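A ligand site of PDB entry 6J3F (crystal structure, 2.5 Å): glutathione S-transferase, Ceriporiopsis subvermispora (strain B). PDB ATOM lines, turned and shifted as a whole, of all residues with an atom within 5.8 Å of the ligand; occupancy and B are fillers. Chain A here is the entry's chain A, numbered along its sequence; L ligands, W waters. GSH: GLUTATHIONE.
The backbone NH (N) of Leu 71 is in hydrogen-bond range of an oxygen (O2) of the ligand (2.8 Å).
The backbone carbonyl oxygen (O) of Leu 71 sits at hydrogen-bond distance from a nitrogen (N2) of the ligand.
O31 of the ligand sits at hydrogen-bond distance from OH of Tyr 68 (2.7 Å).
An oxygen (O11) of the ligand is in hydrogen-bond range of the backbone NH (N) of Ser 86 (2.8 Å).
The side-chain hydroxyl (OG) of Ser 86 sits at hydrogen-bond distance from an oxygen (O12) of the ligand, 2.8 Å away.
An oxygen (O31) of the ligand is in salt-bridge range of the guanidinium group (NH2) of Arg 151, at 2.8 Å.
A nitrogen (N1) of the ligand lies within salt-bridge range of the side-chain carboxylate (OD2) of Asp 85, at 2.8 Å.
The side-chain hydroxyl of Ser 21 sits close to a sulfur (SG2) of the ligand (3.0 Å).
An oxygen (O12) of the ligand lies within salt-bridge range of the side-chain amino group of Lys 26 (3.1 Å).
The side-chain amide oxygen (OD1) of Asn 23 sits close to an oxygen (O12) of the ligand (3.2 Å).
Residues that only touch the ligand: Ile 10, Tyr 45, Ile 48, Tyr 69, Thr 70, Pro 72 and Phe 146.
Along chain A the residues within 4 Å of the ligand span positions 10 to 151.
The nearest printed residue that does not touch the ligand is Pro 22 (4.1 Å).
The backbone carbonyl oxygen (O) of Tyr 68 sits at hydrogen-bond distance from the backbone NH (N) of Thr 60, 3.0 Å away.
The side-chain hydroxyl of Ser 86 lies within hydrogen-bond range of the side-chain hydroxyl of Tyr 206 (2.8 Å).
NH1 of Arg 151 sits at hydrogen-bond distance from OG1 of Thr 150 (2.8 Å).
The side-chain hydroxyl (OG) of Ser 21 sits close to the backbone NH (N) of Asn 23.
The side-chain hydroxyl of Ser 21 lies within hydrogen-bond range of the backbone NH of Thr 24.
The side-chain amino group of Lys 26 sits at hydrogen-bond distance from the side-chain amide oxygen of Asn 23 (2.9 Å).
The side-chain hydroxyl (OG1) of Thr 60 sits at hydrogen-bond distance from the side-chain hydroxyl (OG1) of Thr 70 (2.6 Å).
The backbone carbonyl oxygen of Ile 10 lies within hydrogen-bond range of the indole nitrogen of Trp 20, 2.9 Å away.
Water W1 lies within hydrogen-bond range of O of Pro 72, OG1 of Thr 70, O11 of the ligand, O of Leu 71 and N of Asp 85.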
ATOM      1  N   ILE A  10       1.050  15.361 -33.834  1.00  0.00           N
ATOM      2  CA  ILE A  10       0.109  16.459 -33.956  1.00  0.00           C
ATOM      3  C   ILE A  10       0.878  17.771 -33.768  1.00  0.00           C
ATOM      4  O   ILE A  10       1.457  17.996 -32.697  1.00  0.00           O
ATOM      5  CB  ILE A  10      -1.037  16.355 -32.937  1.00  0.00           C
ATOM      6  CG1 ILE A  10      -1.645  14.958 -32.955  1.00  0.00           C
ATOM      7  CG2 ILE A  10      -2.062  17.421 -33.196  1.00  0.00           C
ATOM      8  CD1 ILE A  10      -2.774  14.780 -31.959  1.00  0.00           C
ATOM      9  N   TRP A  20       4.182  19.067 -28.952  1.00  0.00           N
ATOM     10  CA  TRP A  20       3.552  19.383 -27.670  1.00  0.00           C
ATOM     11  C   TRP A  20       2.826  18.207 -27.029  1.00  0.00           C
ATOM     12  O   TRP A  20       2.616  18.236 -25.814  1.00  0.00           O
ATOM     13  CB  TRP A  20       2.546  20.510 -27.852  1.00  0.00           C
ATOM     14  CG  TRP A  20       1.458  20.059 -28.747  1.00  0.00           C
ATOM     15  CD1 TRP A  20       1.451  20.098 -30.110  1.00  0.00           C
ATOM     16  CD2 TRP A  20       0.221  19.445 -28.351  1.00  0.00           C
ATOM     17  NE1 TRP A  20       0.278  19.551 -30.590  1.00  0.00           N
ATOM     18  CE2 TRP A  20      -0.492  19.162 -29.537  1.00  0.00           C
ATOM     19  CE3 TRP A  20      -0.351  19.123 -27.121  1.00  0.00           C
ATOM     20  CZ2 TRP A  20      -1.760  18.558 -29.509  1.00  0.00           C
ATOM     21  CZ3 TRP A  20      -1.594  18.525 -27.092  1.00  0.00           C
ATOM     22  CH2 TRP A  20      -2.287  18.245 -28.285  1.00  0.00           C
ATOM     23  N   SER A  21       2.414  17.193 -27.779  1.00  0.00           N
ATOM     24  CA  SER A  21       1.478  16.201 -27.259  1.00  0.00           C
ATOM     25  C   SER A  21       2.086  15.405 -26.114  1.00  0.00           C
ATOM     26  O   SER A  21       3.255  14.985 -26.195  1.00  0.00           O
ATOM     27  CB  SER A  21       1.045  15.255 -28.383  1.00  0.00           C
ATOM     28  OG  SER A  21       0.183  14.256 -27.886  1.00  0.00           O
ATOM     29  N   PRO A  22       1.329  15.162 -25.033  1.00  0.00           N
ATOM     30  CA  PRO A  22       1.852  14.269 -23.988  1.00  0.00           C
ATOM     31  C   PRO A  22       2.012  12.838 -24.480  1.00  0.00           C
ATOM     32  O   PRO A  22       3.015  12.187 -24.133  1.00  0.00           O
ATOM     33  CB  PRO A  22       0.779  14.390 -22.892  1.00  0.00           C
ATOM     34  CG  PRO A  22      -0.481  14.713 -23.653  1.00  0.00           C
ATOM     35  CD  PRO A  22      -0.023  15.642 -24.720  1.00  0.00           C
ATOM     36  N   ASN A  23       1.062  12.336 -25.281  1.00  0.00           N
ATOM     37  CA  ASN A  23       1.122  10.941 -25.705  1.00  0.00           C
ATOM     38  C   ASN A  23       2.156  10.730 -26.799  1.00  0.00           C
ATOM     39  O   ASN A  23       2.825   9.684 -26.824  1.00  0.00           O
ATOM     40  CB  ASN A  23      -0.257  10.453 -26.161  1.00  0.00           C
ATOM     41  CG  ASN A  23      -1.209  10.190 -24.989  1.00  0.00           C
ATOM     42  OD1 ASN A  23      -0.983   9.296 -24.168  1.00  0.00           O
ATOM     43  ND2 ASN A  23      -2.284  10.964 -24.920  1.00  0.00           N
ATOM     44  N   THR A  24       2.322  11.702 -27.714  1.00  0.00           N
ATOM     45  CA  THR A  24       3.338  11.489 -28.738  1.00  0.00           C
ATOM     46  C   THR A  24       4.726  11.747 -28.202  1.00  0.00           C
ATOM     47  O   THR A  24       5.693  11.125 -28.667  1.00  0.00           O
ATOM     48  CB  THR A  24       3.097  12.357 -29.979  1.00  0.00           C
ATOM     49  OG1 THR A  24       3.327  13.731 -29.679  1.00  0.00           O
ATOM     50  CG2 THR A  24       1.692  12.148 -30.477  1.00  0.00           C
ATOM     51  N   LYS A  26       5.732  10.731 -25.396  1.00  0.00           N
ATOM     52  CA  LYS A  26       6.153   9.453 -24.835  1.00  0.00           C
ATOM     53  C   LYS A  26       6.886   8.626 -25.888  1.00  0.00           C
ATOM     54  O   LYS A  26       7.980   8.106 -25.621  1.00  0.00           O
ATOM     55  CB  LYS A  26       4.971   8.677 -24.271  1.00  0.00           C
ATOM     56  CG  LYS A  26       4.460   9.215 -22.959  1.00  0.00           C
ATOM     57  CD  LYS A  26       3.338   8.359 -22.419  1.00  0.00           C
ATOM     58  CE  LYS A  26       2.073   8.545 -23.234  1.00  0.00           C
ATOM     59  NZ  LYS A  26       1.026   7.526 -22.951  1.00  0.00           N
ATOM     60  N   TYR A  45      -5.695  17.144 -35.748  1.00  0.00           N
ATOM     61  CA  TYR A  45      -6.688  16.330 -35.076  1.00  0.00           C
ATOM     62  C   TYR A  45      -7.753  15.810 -36.029  1.00  0.00           C
ATOM     63  O   TYR A  45      -7.910  14.585 -36.149  1.00  0.00           O
ATOM     64  CB  TYR A  45      -7.360  17.088 -33.921  1.00  0.00           C
ATOM     65  CG  TYR A  45      -6.719  16.918 -32.558  1.00  0.00           C
ATOM     66  CD1 TYR A  45      -5.663  17.729 -32.162  1.00  0.00           C
ATOM     67  CD2 TYR A  45      -7.199  15.990 -31.644  1.00  0.00           C
ATOM     68  CE1 TYR A  45      -5.083  17.590 -30.903  1.00  0.00           C
ATOM     69  CE2 TYR A  45      -6.634  15.840 -30.378  1.00  0.00           C
ATOM     70  CZ  TYR A  45      -5.574  16.642 -30.014  1.00  0.00           C
ATOM     71  OH  TYR A  45      -5.010  16.517 -28.764  1.00  0.00           O
ATOM     72  N   ILE A  48      -6.758  12.708 -38.036  1.00  0.00           N
ATOM     73  CA  ILE A  48      -6.145  11.531 -37.422  1.00  0.00           C
ATOM     74  C   ILE A  48      -6.867  10.260 -37.860  1.00  0.00           C
ATOM     75  O   ILE A  48      -6.240   9.304 -38.322  1.00  0.00           O
ATOM     76  CB  ILE A  48      -6.133  11.653 -35.891  1.00  0.00           C
ATOM     77  CG1 ILE A  48      -5.136  12.729 -35.437  1.00  0.00           C
ATOM     78  CG2 ILE A  48      -5.856  10.294 -35.286  1.00  0.00           C
ATOM     79  CD1 ILE A  48      -5.201  12.994 -33.955  1.00  0.00           C
ATOM     80  N   THR A  60      -6.954   2.746 -31.000  1.00  0.00           N
ATOM     81  CA  THR A  60      -6.391   2.432 -29.686  1.00  0.00           C
ATOM     82  C   THR A  60      -7.435   2.105 -28.632  1.00  0.00           C
ATOM     83  O   THR A  60      -7.072   1.627 -27.560  1.00  0.00           O
ATOM     84  CB  THR A  60      -5.519   3.564 -29.181  1.00  0.00           C
ATOM     85  OG1 THR A  60      -6.244   4.794 -29.210  1.00  0.00           O
ATOM     86  CG2 THR A  60      -4.288   3.690 -30.050  1.00  0.00           C
ATOM     87  N   TYR A  68     -11.832   4.333 -31.899  1.00  0.00           N
ATOM     88  CA  TYR A  68     -11.273   5.624 -31.519  1.00  0.00           C
ATOM     89  C   TYR A  68      -9.810   5.648 -31.936  1.00  0.00           C
ATOM     90  O   TYR A  68      -8.993   4.871 -31.423  1.00  0.00           O
ATOM     91  CB  TYR A  68     -11.458   5.862 -30.024  1.00  0.00           C
ATOM     92  CG  TYR A  68     -11.014   7.241 -29.581  1.00  0.00           C
ATOM     93  CD1 TYR A  68     -11.229   8.353 -30.378  1.00  0.00           C
ATOM     94  CD2 TYR A  68     -10.402   7.436 -28.353  1.00  0.00           C
ATOM     95  CE1 TYR A  68     -10.818   9.622 -29.976  1.00  0.00           C
ATOM     96  CE2 TYR A  68      -9.994   8.715 -27.941  1.00  0.00           C
ATOM     97  CZ  TYR A  68     -10.201   9.795 -28.744  1.00  0.00           C
ATOM     98  OH  TYR A  68      -9.784  11.043 -28.307  1.00  0.00           O
ATOM     99  N   TYR A  69      -9.473   6.534 -32.878  1.00  0.00           N
ATOM    100  CA  TYR A  69      -8.148   6.600 -33.485  1.00  0.00           C
ATOM    101  C   TYR A  69      -7.343   7.716 -32.814  1.00  0.00           C
ATOM    102  O   TYR A  69      -7.836   8.839 -32.671  1.00  0.00           O
ATOM    103  CB  TYR A  69      -8.243   6.813 -35.007  1.00  0.00           C
ATOM    104  CG  TYR A  69      -8.824   5.628 -35.813  1.00  0.00           C
ATOM    105  CD1 TYR A  69      -8.030   4.544 -36.184  1.00  0.00           C
ATOM    106  CD2 TYR A  69     -10.170   5.596 -36.198  1.00  0.00           C
ATOM    107  CE1 TYR A  69      -8.560   3.469 -36.912  1.00  0.00           C
ATOM    108  CE2 TYR A  69     -10.709   4.525 -36.913  1.00  0.00           C
ATOM    109  CZ  TYR A  69      -9.901   3.465 -37.272  1.00  0.00           C
ATOM    110  OH  TYR A  69     -10.416   2.399 -37.986  1.00  0.00           O
ATOM    111  N   THR A  70      -6.119   7.411 -32.422  1.00  0.00           N
ATOM    112  CA  THR A  70      -5.270   8.373 -31.732  1.00  0.00           C
ATOM    113  C   THR A  70      -3.861   8.350 -32.304  1.00  0.00           C
ATOM    114  O   THR A  70      -3.441   7.422 -33.004  1.00  0.00           O
ATOM    115  CB  THR A  70      -5.187   8.090 -30.233  1.00  0.00           C
ATOM    116  OG1 THR A  70      -4.682   6.770 -30.025  1.00  0.00           O
ATOM    117  CG2 THR A  70      -6.560   8.261 -29.555  1.00  0.00           C
ATOM    118  N   LEU A  71      -3.129   9.409 -31.973  1.00  0.00           N
ATOM    119  CA  LEU A  71      -1.703   9.464 -32.202  1.00  0.00           C
ATOM    120  C   LEU A  71      -1.082   9.303 -30.812  1.00  0.00           C
ATOM    121  O   LEU A  71      -1.743   9.628 -29.824  1.00  0.00           O
ATOM    122  CB  LEU A  71      -1.299  10.777 -32.884  1.00  0.00           C
ATOM    123  CG  LEU A  71      -1.758  10.909 -34.342  1.00  0.00           C
ATOM    124  CD1 LEU A  71      -1.016  12.048 -35.034  1.00  0.00           C
ATOM    125  CD2 LEU A  71      -1.562   9.596 -35.099  1.00  0.00           C
ATOM    126  N   PRO A  72       0.157   8.805 -30.706  1.00  0.00           N
ATOM    127  CA  PRO A  72       1.107   8.533 -31.792  1.00  0.00           C
ATOM    128  C   PRO A  72       0.843   7.242 -32.497  1.00  0.00           C
ATOM    129  O   PRO A  72       0.167   6.390 -31.944  1.00  0.00           O
ATOM    130  CB  PRO A  72       2.451   8.457 -31.060  1.00  0.00           C
ATOM    131  CG  PRO A  72       2.085   7.947 -29.695  1.00  0.00           C
ATOM    132  CD  PRO A  72       0.722   8.494 -29.383  1.00  0.00           C
ATOM    133  N   SER A  84      -0.011   1.473 -33.194  1.00  0.00           N
ATOM    134  CA  SER A  84      -0.679   2.580 -32.537  1.00  0.00           C
ATOM    135  C   SER A  84      -0.641   2.350 -31.045  1.00  0.00           C
ATOM    136  O   SER A  84      -0.604   1.203 -30.579  1.00  0.00           O
ATOM    137  CB  SER A  84      -2.122   2.702 -33.020  1.00  0.00           C
ATOM    138  OG  SER A  84      -2.805   1.480 -32.793  1.00  0.00           O
ATOM    139  N   ASP A  85      -0.676   3.459 -30.298  1.00  0.00           N
ATOM    140  CA  ASP A  85      -0.614   3.532 -28.848  1.00  0.00           C
ATOM    141  C   ASP A  85       0.841   3.518 -28.393  1.00  0.00           C
ATOM    142  O   ASP A  85       1.578   2.591 -28.726  1.00  0.00           O
ATOM    143  CB  ASP A  85      -1.392   2.404 -28.158  1.00  0.00           C
ATOM    144  CG  ASP A  85      -1.480   2.590 -26.652  1.00  0.00           C
ATOM    145  OD1 ASP A  85      -0.452   2.383 -25.969  1.00  0.00           O
ATOM    146  OD2 ASP A  85      -2.573   2.944 -26.140  1.00  0.00           O
ATOM    147  N   SER A  86       1.221   4.533 -27.623  1.00  0.00           N
ATOM    148  CA  SER A  86       2.625   4.706 -27.235  1.00  0.00           C
ATOM    149  C   SER A  86       3.187   3.490 -26.488  1.00  0.00           C
ATOM    150  O   SER A  86       4.321   3.073 -26.741  1.00  0.00           O
ATOM    151  CB  SER A  86       2.774   5.959 -26.387  1.00  0.00           C
ATOM    152  OG  SER A  86       1.932   5.901 -25.254  1.00  0.00           O
ATOM    153  N   ALA A  87       2.402   2.897 -25.579  1.00  0.00           N
ATOM    154  CA  ALA A  87       2.885   1.698 -24.884  1.00  0.00           C
ATOM    155  C   ALA A  87       3.085   0.516 -25.843  1.00  0.00           C
ATOM    156  O   ALA A  87       4.043  -0.250 -25.703  1.00  0.00           O
ATOM    157  CB  ALA A  87       1.945   1.307 -23.742  1.00  0.00           C
ATOM    158  N   PHE A 146     -11.888  21.206 -34.115  1.00  0.00           N
ATOM    159  CA  PHE A 146     -12.160  19.833 -33.690  1.00  0.00           C
ATOM    160  C   PHE A 146     -11.950  19.655 -32.182  1.00  0.00           C
ATOM    161  O   PHE A 146     -12.738  18.978 -31.512  1.00  0.00           O
ATOM    162  CB  PHE A 146     -11.266  18.895 -34.503  1.00  0.00           C
ATOM    163  CG  PHE A 146     -11.466  17.430 -34.233  1.00  0.00           C
ATOM    164  CD1 PHE A 146     -10.938  16.836 -33.083  1.00  0.00           C
ATOM    165  CD2 PHE A 146     -12.133  16.631 -35.149  1.00  0.00           C
ATOM    166  CE1 PHE A 146     -11.096  15.477 -32.839  1.00  0.00           C
ATOM    167  CE2 PHE A 146     -12.294  15.270 -34.914  1.00  0.00           C
ATOM    168  CZ  PHE A 146     -11.785  14.686 -33.761  1.00  0.00           C
ATOM    169  N   THR A 150     -15.161  18.738 -29.597  1.00  0.00           N
ATOM    170  CA  THR A 150     -15.237  17.442 -28.931  1.00  0.00           C
ATOM    171  C   THR A 150     -15.062  17.571 -27.414  1.00  0.00           C
ATOM    172  O   THR A 150     -15.721  16.863 -26.640  1.00  0.00           O
ATOM    173  CB  THR A 150     -14.186  16.501 -29.516  1.00  0.00           C
ATOM    174  OG1 THR A 150     -12.881  17.091 -29.380  1.00  0.00           O
ATOM    175  CG2 THR A 150     -14.478  16.236 -30.986  1.00  0.00           C
ATOM    176  N   ARG A 151     -14.172  18.458 -26.969  1.00  0.00           N
ATOM    177  CA  ARG A 151     -13.911  18.541 -25.534  1.00  0.00           C
ATOM    178  C   ARG A 151     -15.043  19.245 -24.795  1.00  0.00           C
ATOM    179  O   ARG A 151     -15.473  18.783 -23.732  1.00  0.00           O
ATOM    180  CB  ARG A 151     -12.582  19.257 -25.272  1.00  0.00           C
ATOM    181  CG  ARG A 151     -11.373  18.355 -25.262  1.00  0.00           C
ATOM    182  CD  ARG A 151     -11.261  17.551 -26.533  1.00  0.00           C
ATOM    183  NE  ARG A 151     -10.132  16.640 -26.482  1.00  0.00           N
ATOM    184  CZ  ARG A 151      -9.773  15.823 -27.467  1.00  0.00           C
ATOM    185  NH1 ARG A 151     -10.460  15.818 -28.615  1.00  0.00           N
ATOM    186  NH2 ARG A 151      -8.721  15.027 -27.319  1.00  0.00           N
ATOM    187  N   TYR A 206      10.261   2.572 -19.512  1.00  0.00           N
ATOM    188  CA  TYR A 206       9.146   3.270 -20.123  1.00  0.00           C
ATOM    189  C   TYR A 206       8.289   3.970 -19.076  1.00  0.00           C
ATOM    190  O   TYR A 206       7.720   5.022 -19.355  1.00  0.00           O
ATOM    191  CB  TYR A 206       8.325   2.321 -21.008  1.00  0.00           C
ATOM    192  CG  TYR A 206       7.170   2.992 -21.740  1.00  0.00           C
ATOM    193  CD1 TYR A 206       7.389   3.895 -22.786  1.00  0.00           C
ATOM    194  CD2 TYR A 206       5.846   2.724 -21.380  1.00  0.00           C
ATOM    195  CE1 TYR A 206       6.305   4.518 -23.445  1.00  0.00           C
ATOM    196  CE2 TYR A 206       4.783   3.325 -22.030  1.00  0.00           C
ATOM    197  CZ  TYR A 206       5.003   4.216 -23.064  1.00  0.00           C
ATOM    198  OH  TYR A 206       3.911   4.807 -23.681  1.00  0.00           O
HETATM  199  N1  GSH L   1      -3.457   5.420 -25.087  1.00  0.00           N
HETATM  200  CA1 GSH L   1      -2.984   6.261 -26.172  1.00  0.00           C
HETATM  201  C1  GSH L   1      -1.479   6.306 -26.177  1.00  0.00           C
HETATM  202  O11 GSH L   1      -0.871   6.354 -27.284  1.00  0.00           O
HETATM  203  O12 GSH L   1      -0.860   6.274 -25.084  1.00  0.00           O
HETATM  204  CB1 GSH L   1      -3.600   7.653 -26.036  1.00  0.00           C
HETATM  205  CG1 GSH L   1      -3.244   8.498 -27.245  1.00  0.00           C
HETATM  206  CD1 GSH L   1      -4.072   9.765 -27.345  1.00  0.00           C
HETATM  207  OE1 GSH L   1      -5.087   9.913 -26.684  1.00  0.00           O
HETATM  208  N2  GSH L   1      -3.600  10.674 -28.197  1.00  0.00           N
HETATM  209  CA2 GSH L   1      -4.310  11.909 -28.512  1.00  0.00           C
HETATM  210  C2  GSH L   1      -5.143  11.800 -29.761  1.00  0.00           C
HETATM  211  O2  GSH L   1      -4.623  11.474 -30.820  1.00  0.00           O
HETATM  212  CB2 GSH L   1      -3.304  13.042 -28.654  1.00  0.00           C
HETATM  213  SG2 GSH L   1      -2.583  13.531 -27.064  1.00  0.00           S
HETATM  214  N3  GSH L   1      -6.442  12.077 -29.669  1.00  0.00           N
HETATM  215  CA3 GSH L   1      -7.315  12.048 -30.825  1.00  0.00           C
HETATM  216  C3  GSH L   1      -8.655  12.737 -30.606  1.00  0.00           C
HETATM  217  O31 GSH L   1      -8.894  13.280 -29.494  1.00  0.00           O
HETATM  218  O32 GSH L   1      -9.476  12.742 -31.550  1.00  0.00           O
HETATM  219  O   HOH W   1      -1.827   6.564 -30.113  1.00  0.00           O
